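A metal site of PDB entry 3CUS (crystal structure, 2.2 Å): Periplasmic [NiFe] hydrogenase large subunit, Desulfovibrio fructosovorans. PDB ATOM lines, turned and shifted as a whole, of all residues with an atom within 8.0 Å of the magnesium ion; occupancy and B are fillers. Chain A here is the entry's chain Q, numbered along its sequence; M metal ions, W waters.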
ATOM      1  N   PHE A  49      -5.708   0.763 -12.576  1.00  0.00           N
ATOM      2  CA  PHE A  49      -6.095   1.765 -11.568  1.00  0.00           C
ATOM      3  C   PHE A  49      -7.294   2.584 -12.066  1.00  0.00           C
ATOM      4  O   PHE A  49      -7.371   2.981 -13.234  1.00  0.00           O
ATOM      5  CB  PHE A  49      -4.918   2.705 -11.248  1.00  0.00           C
ATOM      6  CG  PHE A  49      -5.245   3.760 -10.208  1.00  0.00           C
ATOM      7  CD1 PHE A  49      -5.106   3.494  -8.849  1.00  0.00           C
ATOM      8  CD2 PHE A  49      -5.718   5.018 -10.590  1.00  0.00           C
ATOM      9  CE1 PHE A  49      -5.410   4.448  -7.894  1.00  0.00           C
ATOM     10  CE2 PHE A  49      -6.019   5.995  -9.641  1.00  0.00           C
ATOM     11  CZ  PHE A  49      -5.863   5.705  -8.289  1.00  0.00           C
ATOM     12  N   GLU A  53     -11.404   6.475  -4.687  1.00  0.00           N
ATOM     13  CA  GLU A  53     -11.145   7.288  -3.487  1.00  0.00           C
ATOM     14  C   GLU A  53     -10.908   8.763  -3.865  1.00  0.00           C
ATOM     15  O   GLU A  53     -11.397   9.661  -3.170  1.00  0.00           O
ATOM     16  CB  GLU A  53      -9.970   6.739  -2.674  1.00  0.00           C
ATOM     17  CG  GLU A  53     -10.201   5.342  -2.076  1.00  0.00           C
ATOM     18  CD  GLU A  53      -8.924   4.583  -1.774  1.00  0.00           C
ATOM     19  OE1 GLU A  53      -7.864   4.878  -2.387  1.00  0.00           O
ATOM     20  OE2 GLU A  53      -8.979   3.670  -0.933  1.00  0.00           O
ATOM     21  N   GLU A 334      -1.764   0.880   5.663  1.00  0.00           N
ATOM     22  CA  GLU A 334      -1.360   0.465   4.323  1.00  0.00           C
ATOM     23  C   GLU A 334      -0.018   1.100   3.929  1.00  0.00           C
ATOM     24  O   GLU A 334       0.173   2.288   4.110  1.00  0.00           O
ATOM     25  CB  GLU A 334      -2.424   0.861   3.299  1.00  0.00           C
ATOM     26  CG  GLU A 334      -3.775   0.241   3.533  1.00  0.00           C
ATOM     27  CD  GLU A 334      -4.762   0.732   2.515  1.00  0.00           C
ATOM     28  OE1 GLU A 334      -5.227   1.888   2.659  1.00  0.00           O
ATOM     29  OE2 GLU A 334      -5.064  -0.036   1.567  1.00  0.00           O
ATOM     30  N   TYR A 341       2.438   4.349  -6.252  1.00  0.00           N
ATOM     31  CA  TYR A 341       2.026   5.611  -5.642  1.00  0.00           C
ATOM     32  C   TYR A 341       3.251   6.425  -5.231  1.00  0.00           C
ATOM     33  O   TYR A 341       4.369   5.904  -5.270  1.00  0.00           O
ATOM     34  CB  TYR A 341       1.088   5.372  -4.450  1.00  0.00           C
ATOM     35  CG  TYR A 341      -0.153   4.587  -4.822  1.00  0.00           C
ATOM     36  CD1 TYR A 341      -0.157   3.200  -4.793  1.00  0.00           C
ATOM     37  CD2 TYR A 341      -1.318   5.235  -5.194  1.00  0.00           C
ATOM     38  CE1 TYR A 341      -1.313   2.481  -5.155  1.00  0.00           C
ATOM     39  CE2 TYR A 341      -2.467   4.528  -5.554  1.00  0.00           C
ATOM     40  CZ  TYR A 341      -2.453   3.155  -5.515  1.00  0.00           C
ATOM     41  OH  TYR A 341      -3.591   2.482  -5.871  1.00  0.00           O
ATOM     42  N   PRO A 350      -6.048   4.013   7.582  1.00  0.00           N
ATOM     43  CA  PRO A 350      -7.013   4.462   6.552  1.00  0.00           C
ATOM     44  C   PRO A 350      -7.710   5.815   6.791  1.00  0.00           C
ATOM     45  O   PRO A 350      -8.075   6.487   5.825  1.00  0.00           O
ATOM     46  CB  PRO A 350      -8.070   3.340   6.560  1.00  0.00           C
ATOM     47  CG  PRO A 350      -7.382   2.169   7.059  1.00  0.00           C
ATOM     48  CD  PRO A 350      -6.379   2.666   8.072  1.00  0.00           C
ATOM     49  N   GLY A 353      -5.492   7.924   5.197  1.00  0.00           N
ATOM     50  CA  GLY A 353      -5.080   7.367   3.921  1.00  0.00           C
ATOM     51  C   GLY A 353      -4.779   8.391   2.827  1.00  0.00           C
ATOM     52  O   GLY A 353      -5.354   9.474   2.788  1.00  0.00           O
ATOM     53  N   VAL A 354      -3.875   8.025   1.934  1.00  0.00           N
ATOM     54  CA  VAL A 354      -3.453   8.894   0.832  1.00  0.00           C
ATOM     55  C   VAL A 354      -3.397   8.062  -0.442  1.00  0.00           C
ATOM     56  O   VAL A 354      -2.841   6.963  -0.444  1.00  0.00           O
ATOM     57  CB  VAL A 354      -2.078   9.565   1.130  1.00  0.00           C
ATOM     58  CG1 VAL A 354      -1.546  10.316  -0.105  1.00  0.00           C
ATOM     59  CG2 VAL A 354      -2.205  10.527   2.306  1.00  0.00           C
ATOM     60  N   THR A 355      -3.990   8.594  -1.503  1.00  0.00           N
ATOM     61  CA  THR A 355      -3.995   7.946  -2.814  1.00  0.00           C
ATOM     62  C   THR A 355      -3.466   8.871  -3.933  1.00  0.00           C
ATOM     63  O   THR A 355      -4.218   9.599  -4.580  1.00  0.00           O
ATOM     64  CB  THR A 355      -5.412   7.399  -3.143  1.00  0.00           C
ATOM     65  OG1 THR A 355      -5.914   6.696  -1.986  1.00  0.00           O
ATOM     66  CG2 THR A 355      -5.357   6.434  -4.309  1.00  0.00           C
ATOM     67  N   TRP A 370      -0.616  -1.690  -8.613  1.00  0.00           N
ATOM     68  CA  TRP A 370      -1.602  -0.658  -8.278  1.00  0.00           C
ATOM     69  C   TRP A 370      -2.258  -0.876  -6.920  1.00  0.00           C
ATOM     70  O   TRP A 370      -2.937   0.033  -6.410  1.00  0.00           O
ATOM     71  CB  TRP A 370      -2.681  -0.542  -9.397  1.00  0.00           C
ATOM     72  CG  TRP A 370      -2.161   0.180 -10.615  1.00  0.00           C
ATOM     73  CD1 TRP A 370      -1.969  -0.339 -11.870  1.00  0.00           C
ATOM     74  CD2 TRP A 370      -1.746   1.556 -10.679  1.00  0.00           C
ATOM     75  NE1 TRP A 370      -1.459   0.631 -12.708  1.00  0.00           N
ATOM     76  CE2 TRP A 370      -1.319   1.807 -12.006  1.00  0.00           C
ATOM     77  CE3 TRP A 370      -1.706   2.616  -9.747  1.00  0.00           C
ATOM     78  CZ2 TRP A 370      -0.850   3.070 -12.420  1.00  0.00           C
ATOM     79  CZ3 TRP A 370      -1.261   3.852 -10.173  1.00  0.00           C
ATOM     80  CH2 TRP A 370      -0.825   4.073 -11.496  1.00  0.00           C
ATOM     81  N   MET A 371      -2.082  -2.059  -6.323  1.00  0.00           N
ATOM     82  CA  MET A 371      -2.616  -2.295  -4.966  1.00  0.00           C
ATOM     83  C   MET A 371      -1.649  -1.714  -3.942  1.00  0.00           C
ATOM     84  O   MET A 371      -0.431  -1.796  -4.127  1.00  0.00           O
ATOM     85  CB  MET A 371      -2.832  -3.786  -4.626  1.00  0.00           C
ATOM     86  CG  MET A 371      -3.955  -4.462  -5.396  1.00  0.00           C
ATOM     87  SD  MET A 371      -4.538  -5.982  -4.582  1.00  0.00           S
ATOM     88  CE  MET A 371      -5.505  -6.723  -5.915  1.00  0.00           C
ATOM     89  N   LYS A 372      -2.202  -1.112  -2.893  1.00  0.00           N
ATOM     90  CA  LYS A 372      -1.458  -0.802  -1.681  1.00  0.00           C
ATOM     91  C   LYS A 372      -1.218  -2.104  -0.911  1.00  0.00           C
ATOM     92  O   LYS A 372      -1.810  -3.137  -1.246  1.00  0.00           O
ATOM     93  CB  LYS A 372      -2.220   0.184  -0.792  1.00  0.00           C
ATOM     94  CG  LYS A 372      -2.499   1.511  -1.448  1.00  0.00           C
ATOM     95  CD  LYS A 372      -3.203   2.446  -0.455  1.00  0.00           C
ATOM     96  CE  LYS A 372      -3.534   3.808  -1.096  1.00  0.00           C
ATOM     97  NZ  LYS A 372      -4.486   4.619  -0.243  1.00  0.00           N
ATOM     98  N   PRO A 374      -1.768  -3.603   2.655  1.00  0.00           N
ATOM     99  CA  PRO A 374      -2.285  -3.491   4.005  1.00  0.00           C
ATOM    100  C   PRO A 374      -1.515  -4.377   4.980  1.00  0.00           C
ATOM    101  O   PRO A 374      -1.149  -5.507   4.651  1.00  0.00           O
ATOM    102  CB  PRO A 374      -3.746  -3.977   3.860  1.00  0.00           C
ATOM    103  CG  PRO A 374      -4.020  -4.016   2.400  1.00  0.00           C
ATOM    104  CD  PRO A 374      -2.707  -4.302   1.758  1.00  0.00           C
ATOM    105  N   SER A 480     -13.334  -2.932   4.756  1.00  0.00           N
ATOM    106  CA  SER A 480     -13.563  -1.726   5.552  1.00  0.00           C
ATOM    107  C   SER A 480     -13.528  -0.453   4.703  1.00  0.00           C
ATOM    108  O   SER A 480     -12.644  -0.271   3.858  1.00  0.00           O
ATOM    109  CB  SER A 480     -12.611  -1.651   6.748  1.00  0.00           C
ATOM    110  OG  SER A 480     -11.253  -1.705   6.350  1.00  0.00           O
ATOM    111  N   TRP A 482     -13.705   3.808   5.170  1.00  0.00           N
ATOM    112  CA  TRP A 482     -13.394   4.772   6.207  1.00  0.00           C
ATOM    113  C   TRP A 482     -13.617   6.198   5.695  1.00  0.00           C
ATOM    114  O   TRP A 482     -13.037   6.592   4.671  1.00  0.00           O
ATOM    115  CB  TRP A 482     -11.947   4.624   6.663  1.00  0.00           C
ATOM    116  CG  TRP A 482     -11.469   3.226   6.965  1.00  0.00           C
ATOM    117  CD1 TRP A 482     -11.212   2.235   6.062  1.00  0.00           C
ATOM    118  CD2 TRP A 482     -11.145   2.681   8.241  1.00  0.00           C
ATOM    119  NE1 TRP A 482     -10.749   1.118   6.689  1.00  0.00           N
ATOM    120  CE2 TRP A 482     -10.699   1.364   8.038  1.00  0.00           C
ATOM    121  CE3 TRP A 482     -11.190   3.187   9.553  1.00  0.00           C
ATOM    122  CZ2 TRP A 482     -10.294   0.531   9.101  1.00  0.00           C
ATOM    123  CZ3 TRP A 482     -10.786   2.354  10.615  1.00  0.00           C
ATOM    124  CH2 TRP A 482     -10.355   1.041  10.374  1.00  0.00           C
ATOM    125  N   PHE A 493     -12.109   9.493   1.866  1.00  0.00           N
ATOM    126  CA  PHE A 493     -12.804   8.215   1.849  1.00  0.00           C
ATOM    127  C   PHE A 493     -11.825   7.157   1.346  1.00  0.00           C
ATOM    128  O   PHE A 493     -11.409   7.199   0.207  1.00  0.00           O
ATOM    129  CB  PHE A 493     -14.066   8.277   0.955  1.00  0.00           C
ATOM    130  CG  PHE A 493     -15.087   7.199   1.265  1.00  0.00           C
ATOM    131  CD1 PHE A 493     -14.860   5.871   0.929  1.00  0.00           C
ATOM    132  CD2 PHE A 493     -16.297   7.540   1.850  1.00  0.00           C
ATOM    133  CE1 PHE A 493     -15.836   4.876   1.217  1.00  0.00           C
ATOM    134  CE2 PHE A 493     -17.263   6.549   2.137  1.00  0.00           C
ATOM    135  CZ  PHE A 493     -17.026   5.229   1.822  1.00  0.00           C
ATOM    136  N   GLN A 494     -11.487   6.205   2.200  1.00  0.00           N
ATOM    137  CA  GLN A 494     -10.534   5.149   1.876  1.00  0.00           C
ATOM    138  C   GLN A 494     -11.229   3.803   1.969  1.00  0.00           C
ATOM    139  O   GLN A 494     -11.947   3.532   2.935  1.00  0.00           O
ATOM    140  CB  GLN A 494      -9.362   5.193   2.846  1.00  0.00           C
ATOM    141  CG  GLN A 494      -8.529   6.472   2.759  1.00  0.00           C
ATOM    142  CD  GLN A 494      -7.737   6.516   1.490  1.00  0.00           C
ATOM    143  OE1 GLN A 494      -7.188   5.507   1.063  1.00  0.00           O
ATOM    144  NE2 GLN A 494      -7.698   7.674   0.854  1.00  0.00           N
ATOM    145  N   LEU A 495     -10.991   2.972   0.955  1.00  0.00           N
ATOM    146  CA  LEU A 495     -11.372   1.569   0.947  1.00  0.00           C
ATOM    147  C   LEU A 495     -10.136   0.725   1.198  1.00  0.00           C
ATOM    148  O   LEU A 495      -9.087   0.959   0.606  1.00  0.00           O
ATOM    149  CB  LEU A 495     -11.926   1.174  -0.435  1.00  0.00           C
ATOM    150  CG  LEU A 495     -13.234   1.770  -0.939  1.00  0.00           C
ATOM    151  CD1 LEU A 495     -13.127   3.227  -1.311  1.00  0.00           C
ATOM    152  CD2 LEU A 495     -13.781   0.937  -2.140  1.00  0.00           C
ATOM    153  N   VAL A 496     -10.289  -0.267   2.069  1.00  0.00           N
ATOM    154  CA  VAL A 496      -9.294  -1.330   2.273  1.00  0.00           C
ATOM    155  C   VAL A 496     -10.040  -2.649   2.143  1.00  0.00           C
ATOM    156  O   VAL A 496     -10.898  -2.956   2.959  1.00  0.00           O
ATOM    157  CB  VAL A 496      -8.635  -1.230   3.675  1.00  0.00           C
ATOM    158  CG1 VAL A 496      -7.560  -2.325   3.839  1.00  0.00           C
ATOM    159  CG2 VAL A 496      -8.044   0.172   3.897  1.00  0.00           C
ATOM    160  N   VAL A 497      -9.677  -3.442   1.127  1.00  0.00           N
ATOM    161  CA  VAL A 497     -10.556  -4.463   0.571  1.00  0.00           C
ATOM    162  C   VAL A 497      -9.896  -5.821   0.708  1.00  0.00           C
ATOM    163  O   VAL A 497      -8.659  -5.885   0.780  1.00  0.00           O
ATOM    164  CB  VAL A 497     -10.882  -4.111  -0.928  1.00  0.00           C
ATOM    165  CG1 VAL A 497     -12.075  -4.930  -1.458  1.00  0.00           C
ATOM    166  CG2 VAL A 497     -11.200  -2.629  -1.033  1.00  0.00           C
ATOM    167  N   THR A 500      -7.020  -6.549  -1.450  1.00  0.00           N
ATOM    168  CA  THR A 500      -5.855  -5.708  -1.138  1.00  0.00           C
ATOM    169  C   THR A 500      -5.013  -6.426  -0.069  1.00  0.00           C
ATOM    170  O   THR A 500      -3.794  -6.535  -0.229  1.00  0.00           O
ATOM    171  CB  THR A 500      -6.213  -4.284  -0.649  1.00  0.00           C
ATOM    172  OG1 THR A 500      -7.452  -3.838  -1.245  1.00  0.00           O
ATOM    173  CG2 THR A 500      -5.082  -3.308  -1.027  1.00  0.00           C
ATOM    174  N   CYS A 546     -11.622  -4.661  -7.002  1.00  0.00           N
ATOM    175  CA  CYS A 546     -11.779  -4.525  -5.538  1.00  0.00           C
ATOM    176  C   CYS A 546     -10.467  -4.111  -4.869  1.00  0.00           C
ATOM    177  O   CYS A 546     -10.407  -3.133  -4.110  1.00  0.00           O
ATOM    178  CB  CYS A 546     -12.235  -5.846  -4.952  1.00  0.00           C
ATOM    179  SG  CYS A 546     -13.977  -6.006  -4.660  1.00  0.00           S
ATOM    180  N   GLY A 547      -9.405  -4.854  -5.117  1.00  0.00           N
ATOM    181  CA  GLY A 547      -8.150  -4.616  -4.411  1.00  0.00           C
ATOM    182  C   GLY A 547      -7.513  -3.235  -4.674  1.00  0.00           C
ATOM    183  O   GLY A 547      -6.935  -2.662  -3.776  1.00  0.00           O
ATOM    184  N   VAL A 548      -7.663  -2.721  -5.880  1.00  0.00           N
ATOM    185  CA  VAL A 548      -7.117  -1.434  -6.302  1.00  0.00           C
ATOM    186  C   VAL A 548      -8.107  -0.276  -6.138  1.00  0.00           C
ATOM    187  O   VAL A 548      -7.718   0.804  -5.668  1.00  0.00           O
ATOM    188  CB  VAL A 548      -6.714  -1.466  -7.814  1.00  0.00           C
ATOM    189  CG1 VAL A 548      -6.203  -0.110  -8.258  1.00  0.00           C
ATOM    190  CG2 VAL A 548      -5.713  -2.567  -8.113  1.00  0.00           C
ATOM    191  N   HIS A 549      -9.377  -0.508  -6.531  1.00  0.00           N
ATOM    192  CA  HIS A 549     -10.424   0.529  -6.598  1.00  0.00           C
ATOM    193  C   HIS A 549      -9.897   1.835  -7.260  1.00  0.00           C
ATOM    194  O   HIS A 549     -10.155   2.958  -6.816  1.00  0.00           O
ATOM    195  CB  HIS A 549     -11.148   0.762  -5.244  1.00  0.00           C
ATOM    196  CG  HIS A 549     -10.247   0.638  -4.038  1.00  0.00           C
ATOM    197  ND1 HIS A 549      -9.772  -0.573  -3.586  1.00  0.00           N
ATOM    198  CD2 HIS A 549      -9.717   1.578  -3.216  1.00  0.00           C
ATOM    199  CE1 HIS A 549      -8.997  -0.376  -2.534  1.00  0.00           C
ATOM    200  NE2 HIS A 549      -8.949   0.923  -2.278  1.00  0.00           N
ATOM    201  OXT HIS A 549      -9.214   1.799  -8.281  1.00  0.00           O
HETATM  202 MG    MG M   1      -7.681   1.900  -0.760  1.00  0.00          MG
HETATM  203  O   HOH W   1      -6.379   2.832  -2.038  1.00  0.00           O
HETATM  204  O   HOH W   2      -6.509   0.288  -0.505  1.00  0.00           O
HETATM  205  O   HOH W   3      -6.888   2.827   0.792  1.00  0.00           O
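The side-chain amide oxygen (OE1) of Gln 494 sits close to the side-chain carboxylate (OE2) of Glu 53 (3.3 Å).
OE1 of Glu 53 is in hydrogen-bond range of OG1 of Thr 355 (2.7 Å).
A ring nitrogen (ND1) of His 549 sits at hydrogen-bond distance from the backbone carbonyl oxygen of Cys 546, at 2.7 Å.
Three residues have an atom within 4 Å of the magnesium ion: Glu 53, Leu 495 and His 549.
The magnesium ion is bound by water W3 (2.0 Å), water W2 (2.0 Å), water W1 (2.0 Å), the backbone carbonyl oxygen of Leu 495 (2.2 Å), the side-chain carboxylate of Glu 53 (2.2 Å) and a ring nitrogen (NE2) of His 549 (2.2 Å).
The magnesium ion has six donor atoms within binding distance.
Water W3 lies within hydrogen-bond range of the side-chain carboxylate of Glu 334, the side-chain amide oxygen of Gln 494 and the side-chain amino group of Lys 372.
Water W1 bridges OE1 of Glu 53 (2.6 Å) and NZ of Lys 372 (3.2 Å).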
